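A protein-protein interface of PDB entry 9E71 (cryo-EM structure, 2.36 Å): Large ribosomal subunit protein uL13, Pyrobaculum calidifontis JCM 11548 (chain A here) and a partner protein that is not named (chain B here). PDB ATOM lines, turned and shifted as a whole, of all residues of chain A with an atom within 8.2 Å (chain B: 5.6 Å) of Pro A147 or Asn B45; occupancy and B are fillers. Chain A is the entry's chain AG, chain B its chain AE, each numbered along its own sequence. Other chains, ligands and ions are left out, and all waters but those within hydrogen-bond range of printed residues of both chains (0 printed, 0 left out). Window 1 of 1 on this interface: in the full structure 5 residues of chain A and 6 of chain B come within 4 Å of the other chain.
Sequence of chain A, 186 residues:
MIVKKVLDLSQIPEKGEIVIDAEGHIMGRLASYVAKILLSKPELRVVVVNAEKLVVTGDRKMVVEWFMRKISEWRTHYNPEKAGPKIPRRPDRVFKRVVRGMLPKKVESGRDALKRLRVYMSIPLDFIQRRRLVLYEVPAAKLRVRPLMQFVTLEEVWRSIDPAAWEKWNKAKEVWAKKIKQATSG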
ATOM      1  N   ARG A 144      27.168  31.753 -23.161  1.00  0.00           N
ATOM      2  CA  ARG A 144      26.268  30.657 -23.493  1.00  0.00           C
ATOM      3  C   ARG A 144      25.605  30.188 -22.207  1.00  0.00           C
ATOM      4  O   ARG A 144      26.244  29.549 -21.368  1.00  0.00           O
ATOM      5  CB  ARG A 144      27.025  29.520 -24.170  1.00  0.00           C
ATOM      6  CG  ARG A 144      26.130  28.458 -24.776  1.00  0.00           C
ATOM      7  CD  ARG A 144      26.948  27.348 -25.400  1.00  0.00           C
ATOM      8  NE  ARG A 144      26.803  26.087 -24.684  1.00  0.00           N
ATOM      9  CZ  ARG A 144      27.808  25.274 -24.394  1.00  0.00           C
ATOM     10  NH1 ARG A 144      29.054  25.571 -24.722  1.00  0.00           N
ATOM     11  NH2 ARG A 144      27.557  24.135 -23.755  1.00  0.00           N
ATOM     12  N   VAL A 145      24.322  30.507 -22.048  1.00  0.00           N
ATOM     13  CA  VAL A 145      23.628  30.189 -20.809  1.00  0.00           C
ATOM     14  C   VAL A 145      23.388  28.689 -20.727  1.00  0.00           C
ATOM     15  O   VAL A 145      22.916  28.061 -21.683  1.00  0.00           O
ATOM     16  CB  VAL A 145      22.309  30.968 -20.709  1.00  0.00           C
ATOM     17  CG1 VAL A 145      21.487  30.775 -21.967  1.00  0.00           C
ATOM     18  CG2 VAL A 145      21.533  30.517 -19.486  1.00  0.00           C
ATOM     19  N   ARG A 146      23.719  28.108 -19.583  1.00  0.00           N
ATOM     20  CA  ARG A 146      23.490  26.704 -19.308  1.00  0.00           C
ATOM     21  C   ARG A 146      22.845  26.564 -17.940  1.00  0.00           C
ATOM     22  O   ARG A 146      23.012  27.435 -17.082  1.00  0.00           O
ATOM     23  CB  ARG A 146      24.799  25.908 -19.346  1.00  0.00           C
ATOM     24  CG  ARG A 146      25.110  25.328 -20.703  1.00  0.00           C
ATOM     25  CD  ARG A 146      26.597  25.319 -20.975  1.00  0.00           C
ATOM     26  NE  ARG A 146      27.200  26.635 -20.821  1.00  0.00           N
ATOM     27  CZ  ARG A 146      28.495  26.878 -20.953  1.00  0.00           C
ATOM     28  NH1 ARG A 146      29.353  25.914 -21.237  1.00  0.00           N
ATOM     29  NH2 ARG A 146      28.941  28.121 -20.804  1.00  0.00           N
ATOM     30  N   PRO A 147      22.086  25.494 -17.718  1.00  0.00           N
ATOM     31  CA  PRO A 147      21.442  25.306 -16.413  1.00  0.00           C
ATOM     32  C   PRO A 147      22.473  25.100 -15.314  1.00  0.00           C
ATOM     33  O   PRO A 147      23.549  24.543 -15.536  1.00  0.00           O
ATOM     34  CB  PRO A 147      20.577  24.056 -16.605  1.00  0.00           C
ATOM     35  CG  PRO A 147      20.993  23.448 -17.878  1.00  0.00           C
ATOM     36  CD  PRO A 147      21.740  24.446 -18.689  1.00  0.00           C
ATOM     37  N   LEU A 148      22.136  25.584 -14.122  1.00  0.00           N
ATOM     38  CA  LEU A 148      22.983  25.466 -12.938  1.00  0.00           C
ATOM     39  C   LEU A 148      24.312  26.202 -13.085  1.00  0.00           C
ATOM     40  O   LEU A 148      25.284  25.864 -12.408  1.00  0.00           O
ATOM     41  CB  LEU A 148      23.239  23.998 -12.583  1.00  0.00           C
ATOM     42  CG  LEU A 148      22.056  23.128 -12.154  1.00  0.00           C
ATOM     43  CD1 LEU A 148      22.552  21.778 -11.685  1.00  0.00           C
ATOM     44  CD2 LEU A 148      21.254  23.800 -11.064  1.00  0.00           C
ATOM     45  N   MET A 149      24.386  27.206 -13.951  1.00  0.00           N
ATOM     46  CA  MET A 149      25.593  28.007 -14.090  1.00  0.00           C
ATOM     47  C   MET A 149      25.495  29.275 -13.255  1.00  0.00           C
ATOM     48  O   MET A 149      24.415  29.838 -13.067  1.00  0.00           O
ATOM     49  CB  MET A 149      25.850  28.373 -15.550  1.00  0.00           C
ATOM     50  CG  MET A 149      27.319  28.556 -15.864  1.00  0.00           C
ATOM     51  SD  MET A 149      27.782  28.076 -17.534  1.00  0.00           S
ATOM     52  CE  MET A 149      29.144  29.207 -17.816  1.00  0.00           C
ATOM     53  N   GLN A 150      26.643  29.722 -12.757  1.00  0.00           N
ATOM     54  CA  GLN A 150      26.724  30.852 -11.845  1.00  0.00           C
ATOM     55  C   GLN A 150      27.345  32.043 -12.552  1.00  0.00           C
ATOM     56  O   GLN A 150      28.414  31.923 -13.158  1.00  0.00           O
ATOM     57  CB  GLN A 150      27.546  30.495 -10.607  1.00  0.00           C
ATOM     58  CG  GLN A 150      26.974  29.352  -9.811  1.00  0.00           C
ATOM     59  CD  GLN A 150      25.644  29.703  -9.200  1.00  0.00           C
ATOM     60  OE1 GLN A 150      24.597  29.475  -9.799  1.00  0.00           O
ATOM     61  NE2 GLN A 150      25.675  30.263  -8.000  1.00  0.00           N
ATOM     62  N   PHE A 151      26.678  33.187 -12.469  1.00  0.00           N
ATOM     63  CA  PHE A 151      27.236  34.422 -12.995  1.00  0.00           C
ATOM     64  C   PHE A 151      26.496  35.589 -12.364  1.00  0.00           C
ATOM     65  O   PHE A 151      25.390  35.434 -11.842  1.00  0.00           O
ATOM     66  CB  PHE A 151      27.161  34.476 -14.526  1.00  0.00           C
ATOM     67  CG  PHE A 151      25.766  34.544 -15.070  1.00  0.00           C
ATOM     68  CD1 PHE A 151      25.208  35.753 -15.438  1.00  0.00           C
ATOM     69  CD2 PHE A 151      25.017  33.396 -15.230  1.00  0.00           C
ATOM     70  CE1 PHE A 151      23.929  35.815 -15.937  1.00  0.00           C
ATOM     71  CE2 PHE A 151      23.737  33.454 -15.731  1.00  0.00           C
ATOM     72  CZ  PHE A 151      23.195  34.664 -16.086  1.00  0.00           C
ATOM     73  N   PHE B  26      16.133  29.060 -19.130  1.00  0.00           N
ATOM     74  CA  PHE B  26      15.933  27.866 -18.317  1.00  0.00           C
ATOM     75  C   PHE B  26      15.098  28.162 -17.079  1.00  0.00           C
ATOM     76  O   PHE B  26      15.210  27.443 -16.080  1.00  0.00           O
ATOM     77  CB  PHE B  26      17.275  27.254 -17.902  1.00  0.00           C
ATOM     78  CG  PHE B  26      18.148  26.882 -19.056  1.00  0.00           C
ATOM     79  CD1 PHE B  26      17.970  25.686 -19.717  1.00  0.00           C
ATOM     80  CD2 PHE B  26      19.130  27.746 -19.500  1.00  0.00           C
ATOM     81  CE1 PHE B  26      18.763  25.351 -20.787  1.00  0.00           C
ATOM     82  CE2 PHE B  26      19.928  27.412 -20.571  1.00  0.00           C
ATOM     83  CZ  PHE B  26      19.744  26.212 -21.214  1.00  0.00           C
ATOM     84  N   ASP B  27      14.268  29.195 -17.119  1.00  0.00           N
ATOM     85  CA  ASP B  27      13.472  29.609 -15.977  1.00  0.00           C
ATOM     86  C   ASP B  27      12.015  29.229 -16.190  1.00  0.00           C
ATOM     87  O   ASP B  27      11.528  29.201 -17.323  1.00  0.00           O
ATOM     88  CB  ASP B  27      13.590  31.115 -15.749  1.00  0.00           C
ATOM     89  CG  ASP B  27      14.982  31.528 -15.339  1.00  0.00           C
ATOM     90  OD1 ASP B  27      15.823  31.772 -16.227  1.00  0.00           O
ATOM     91  OD2 ASP B  27      15.238  31.608 -14.122  1.00  0.00           O
ATOM     92  N   PHE B  43      11.163  28.403 -10.603  1.00  0.00           N
ATOM     93  CA  PHE B  43      12.269  27.461 -10.742  1.00  0.00           C
ATOM     94  C   PHE B  43      13.261  28.095 -11.707  1.00  0.00           C
ATOM     95  O   PHE B  43      13.021  28.128 -12.916  1.00  0.00           O
ATOM     96  CB  PHE B  43      11.784  26.105 -11.242  1.00  0.00           C
ATOM     97  CG  PHE B  43      10.791  25.444 -10.334  1.00  0.00           C
ATOM     98  CD1 PHE B  43       9.437  25.663 -10.493  1.00  0.00           C
ATOM     99  CD2 PHE B  43      11.212  24.606  -9.322  1.00  0.00           C
ATOM    100  CE1 PHE B  43       8.525  25.059  -9.661  1.00  0.00           C
ATOM    101  CE2 PHE B  43      10.301  23.999  -8.489  1.00  0.00           C
ATOM    102  CZ  PHE B  43       8.957  24.226  -8.660  1.00  0.00           C
ATOM    103  N   LYS B  44      14.373  28.593 -11.183  1.00  0.00           N
ATOM    104  CA  LYS B  44      15.320  29.364 -11.971  1.00  0.00           C
ATOM    105  C   LYS B  44      16.596  28.574 -12.219  1.00  0.00           C
ATOM    106  O   LYS B  44      17.091  27.869 -11.338  1.00  0.00           O
ATOM    107  CB  LYS B  44      15.657  30.678 -11.270  1.00  0.00           C
ATOM    108  CG  LYS B  44      14.439  31.446 -10.798  1.00  0.00           C
ATOM    109  CD  LYS B  44      14.816  32.464  -9.742  1.00  0.00           C
ATOM    110  CE  LYS B  44      13.893  32.381  -8.545  1.00  0.00           C
ATOM    111  NZ  LYS B  44      14.639  32.509  -7.265  1.00  0.00           N
ATOM    112  N   ASN B  45      17.126  28.714 -13.435  1.00  0.00           N
ATOM    113  CA  ASN B  45      18.400  28.110 -13.824  1.00  0.00           C
ATOM    114  C   ASN B  45      18.342  26.591 -13.721  1.00  0.00           C
ATOM    115  O   ASN B  45      19.283  25.939 -13.270  1.00  0.00           O
ATOM    116  CB  ASN B  45      19.544  28.671 -12.982  1.00  0.00           C
ATOM    117  CG  ASN B  45      20.711  29.139 -13.823  1.00  0.00           C
ATOM    118  OD1 ASN B  45      20.586  29.317 -15.033  1.00  0.00           O
ATOM    119  ND2 ASN B  45      21.850  29.360 -13.182  1.00  0.00           N
ATOM    120  N   THR B  46      17.224  26.025 -14.147  1.00  0.00           N
ATOM    121  CA  THR B  46      17.045  24.603 -13.909  1.00  0.00           C
ATOM    122  C   THR B  46      17.253  23.809 -15.186  1.00  0.00           C
ATOM    123  O   THR B  46      16.871  24.262 -16.270  1.00  0.00           O
ATOM    124  CB  THR B  46      15.641  24.325 -13.382  1.00  0.00           C
ATOM    125  OG1 THR B  46      14.766  24.079 -14.485  1.00  0.00           O
ATOM    126  CG2 THR B  46      15.135  25.528 -12.638  1.00  0.00           C
ATOM    127  N   PRO B  47      17.862  22.628 -15.083  1.00  0.00           N
ATOM    128  CA  PRO B  47      17.929  21.731 -16.241  1.00  0.00           C
ATOM    129  C   PRO B  47      16.643  20.971 -16.483  1.00  0.00           C
ATOM    130  O   PRO B  47      16.470  20.412 -17.575  1.00  0.00           O
ATOM    131  CB  PRO B  47      19.068  20.779 -15.871  1.00  0.00           C
ATOM    132  CG  PRO B  47      19.056  20.751 -14.394  1.00  0.00           C
ATOM    133  CD  PRO B  47      18.592  22.095 -13.923  1.00  0.00           C
ATOM    134  N   GLU B  68      21.983  16.867 -11.740  1.00  0.00           N
ATOM    135  CA  GLU B  68      20.791  17.281 -12.467  1.00  0.00           C
ATOM    136  C   GLU B  68      19.666  16.274 -12.296  1.00  0.00           C
ATOM    137  O   GLU B  68      18.494  16.651 -12.210  1.00  0.00           O
ATOM    138  CB  GLU B  68      21.116  17.468 -13.945  1.00  0.00           C
ATOM    139  CG  GLU B  68      22.002  18.655 -14.225  1.00  0.00           C
ATOM    140  CD  GLU B  68      23.113  18.326 -15.190  1.00  0.00           C
ATOM    141  OE1 GLU B  68      23.972  17.489 -14.843  1.00  0.00           O
ATOM    142  OE2 GLU B  68      23.127  18.901 -16.297  1.00  0.00           O
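Printed residues of chain B within 4 Å of Pro A147: Phe B26, Asn B45, Thr B46 and Pro B47.
Of the printed residues of chain A, Asn B45 touches Arg A146 (3.7 Å), Pro A147 (3.9 Å), Leu A148 (3.0 Å) and Met A149 (2.6 Å).
Of the printed residues of chain B, Leu A148 touches Asn B45 (3.0 Å).
Of the printed residues of chain B, Arg A146 touches Phe B26 and Asn B45.
Of the printed residues of chain A, Pro B47 touches Pro A147 (3.4 Å).
Of the printed residues of chain A, Phe B26 touches Val A145 (3.3 Å), Arg A146 (3.8 Å) and Pro A147 (3.7 Å).
Arg A144 touches none of the printed residues of chain B.
Phe A151 touches none of the printed residues of chain B.
The nearest residue of chain A that does not touch Asn B45 is Gln A150 (4.4 Å).
The nearest printed residue of chain A that does not touch Phe B26 is Leu A148 (6.4 Å).
The guanidinium group (NH2) of Arg A146 lies close to the side-chain sulfur (SD) of Met A149 (3.5 Å).
The backbone carbonyl oxygen (O) of Arg A144 is in hydrogen-bond range of the guanidinium group (NH2) of Arg A146 (3.1 Å).
The backbone NH (N) of Thr B46 lies within hydrogen-bond range of the backbone carbonyl oxygen (O) of Phe B26 (3.1 Å).
Of the 8 printed residues of chain A, 5 touch a printed residue of chain B.
Of the 8 printed residues of chain B, 4 touch a printed residue of chain A.
Among the printed residues, no Asp or Glu carboxylate lies within 4 Å of a Lys or Arg side-chain nitrogen of the other chain.
The backbone carbonyl oxygen (O) of Asn B45 is in hydrogen-bond range of the backbone NH (N) of Leu A148, 3.0 Å away.
The side-chain amide nitrogen of Asn B45 sits at hydrogen-bond distance from the backbone carbonyl oxygen of Met A149 (2.6 Å).
Among the printed residues, pairs that only touch across the chains: Val A145 with Phe B26, Arg A146 with Phe B26, Arg A146 with Asn B45, Pro A147 with Phe B26, Pro A147 with Asn B45, Pro A147 with Thr B46 and Pro A147 with Pro B47.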
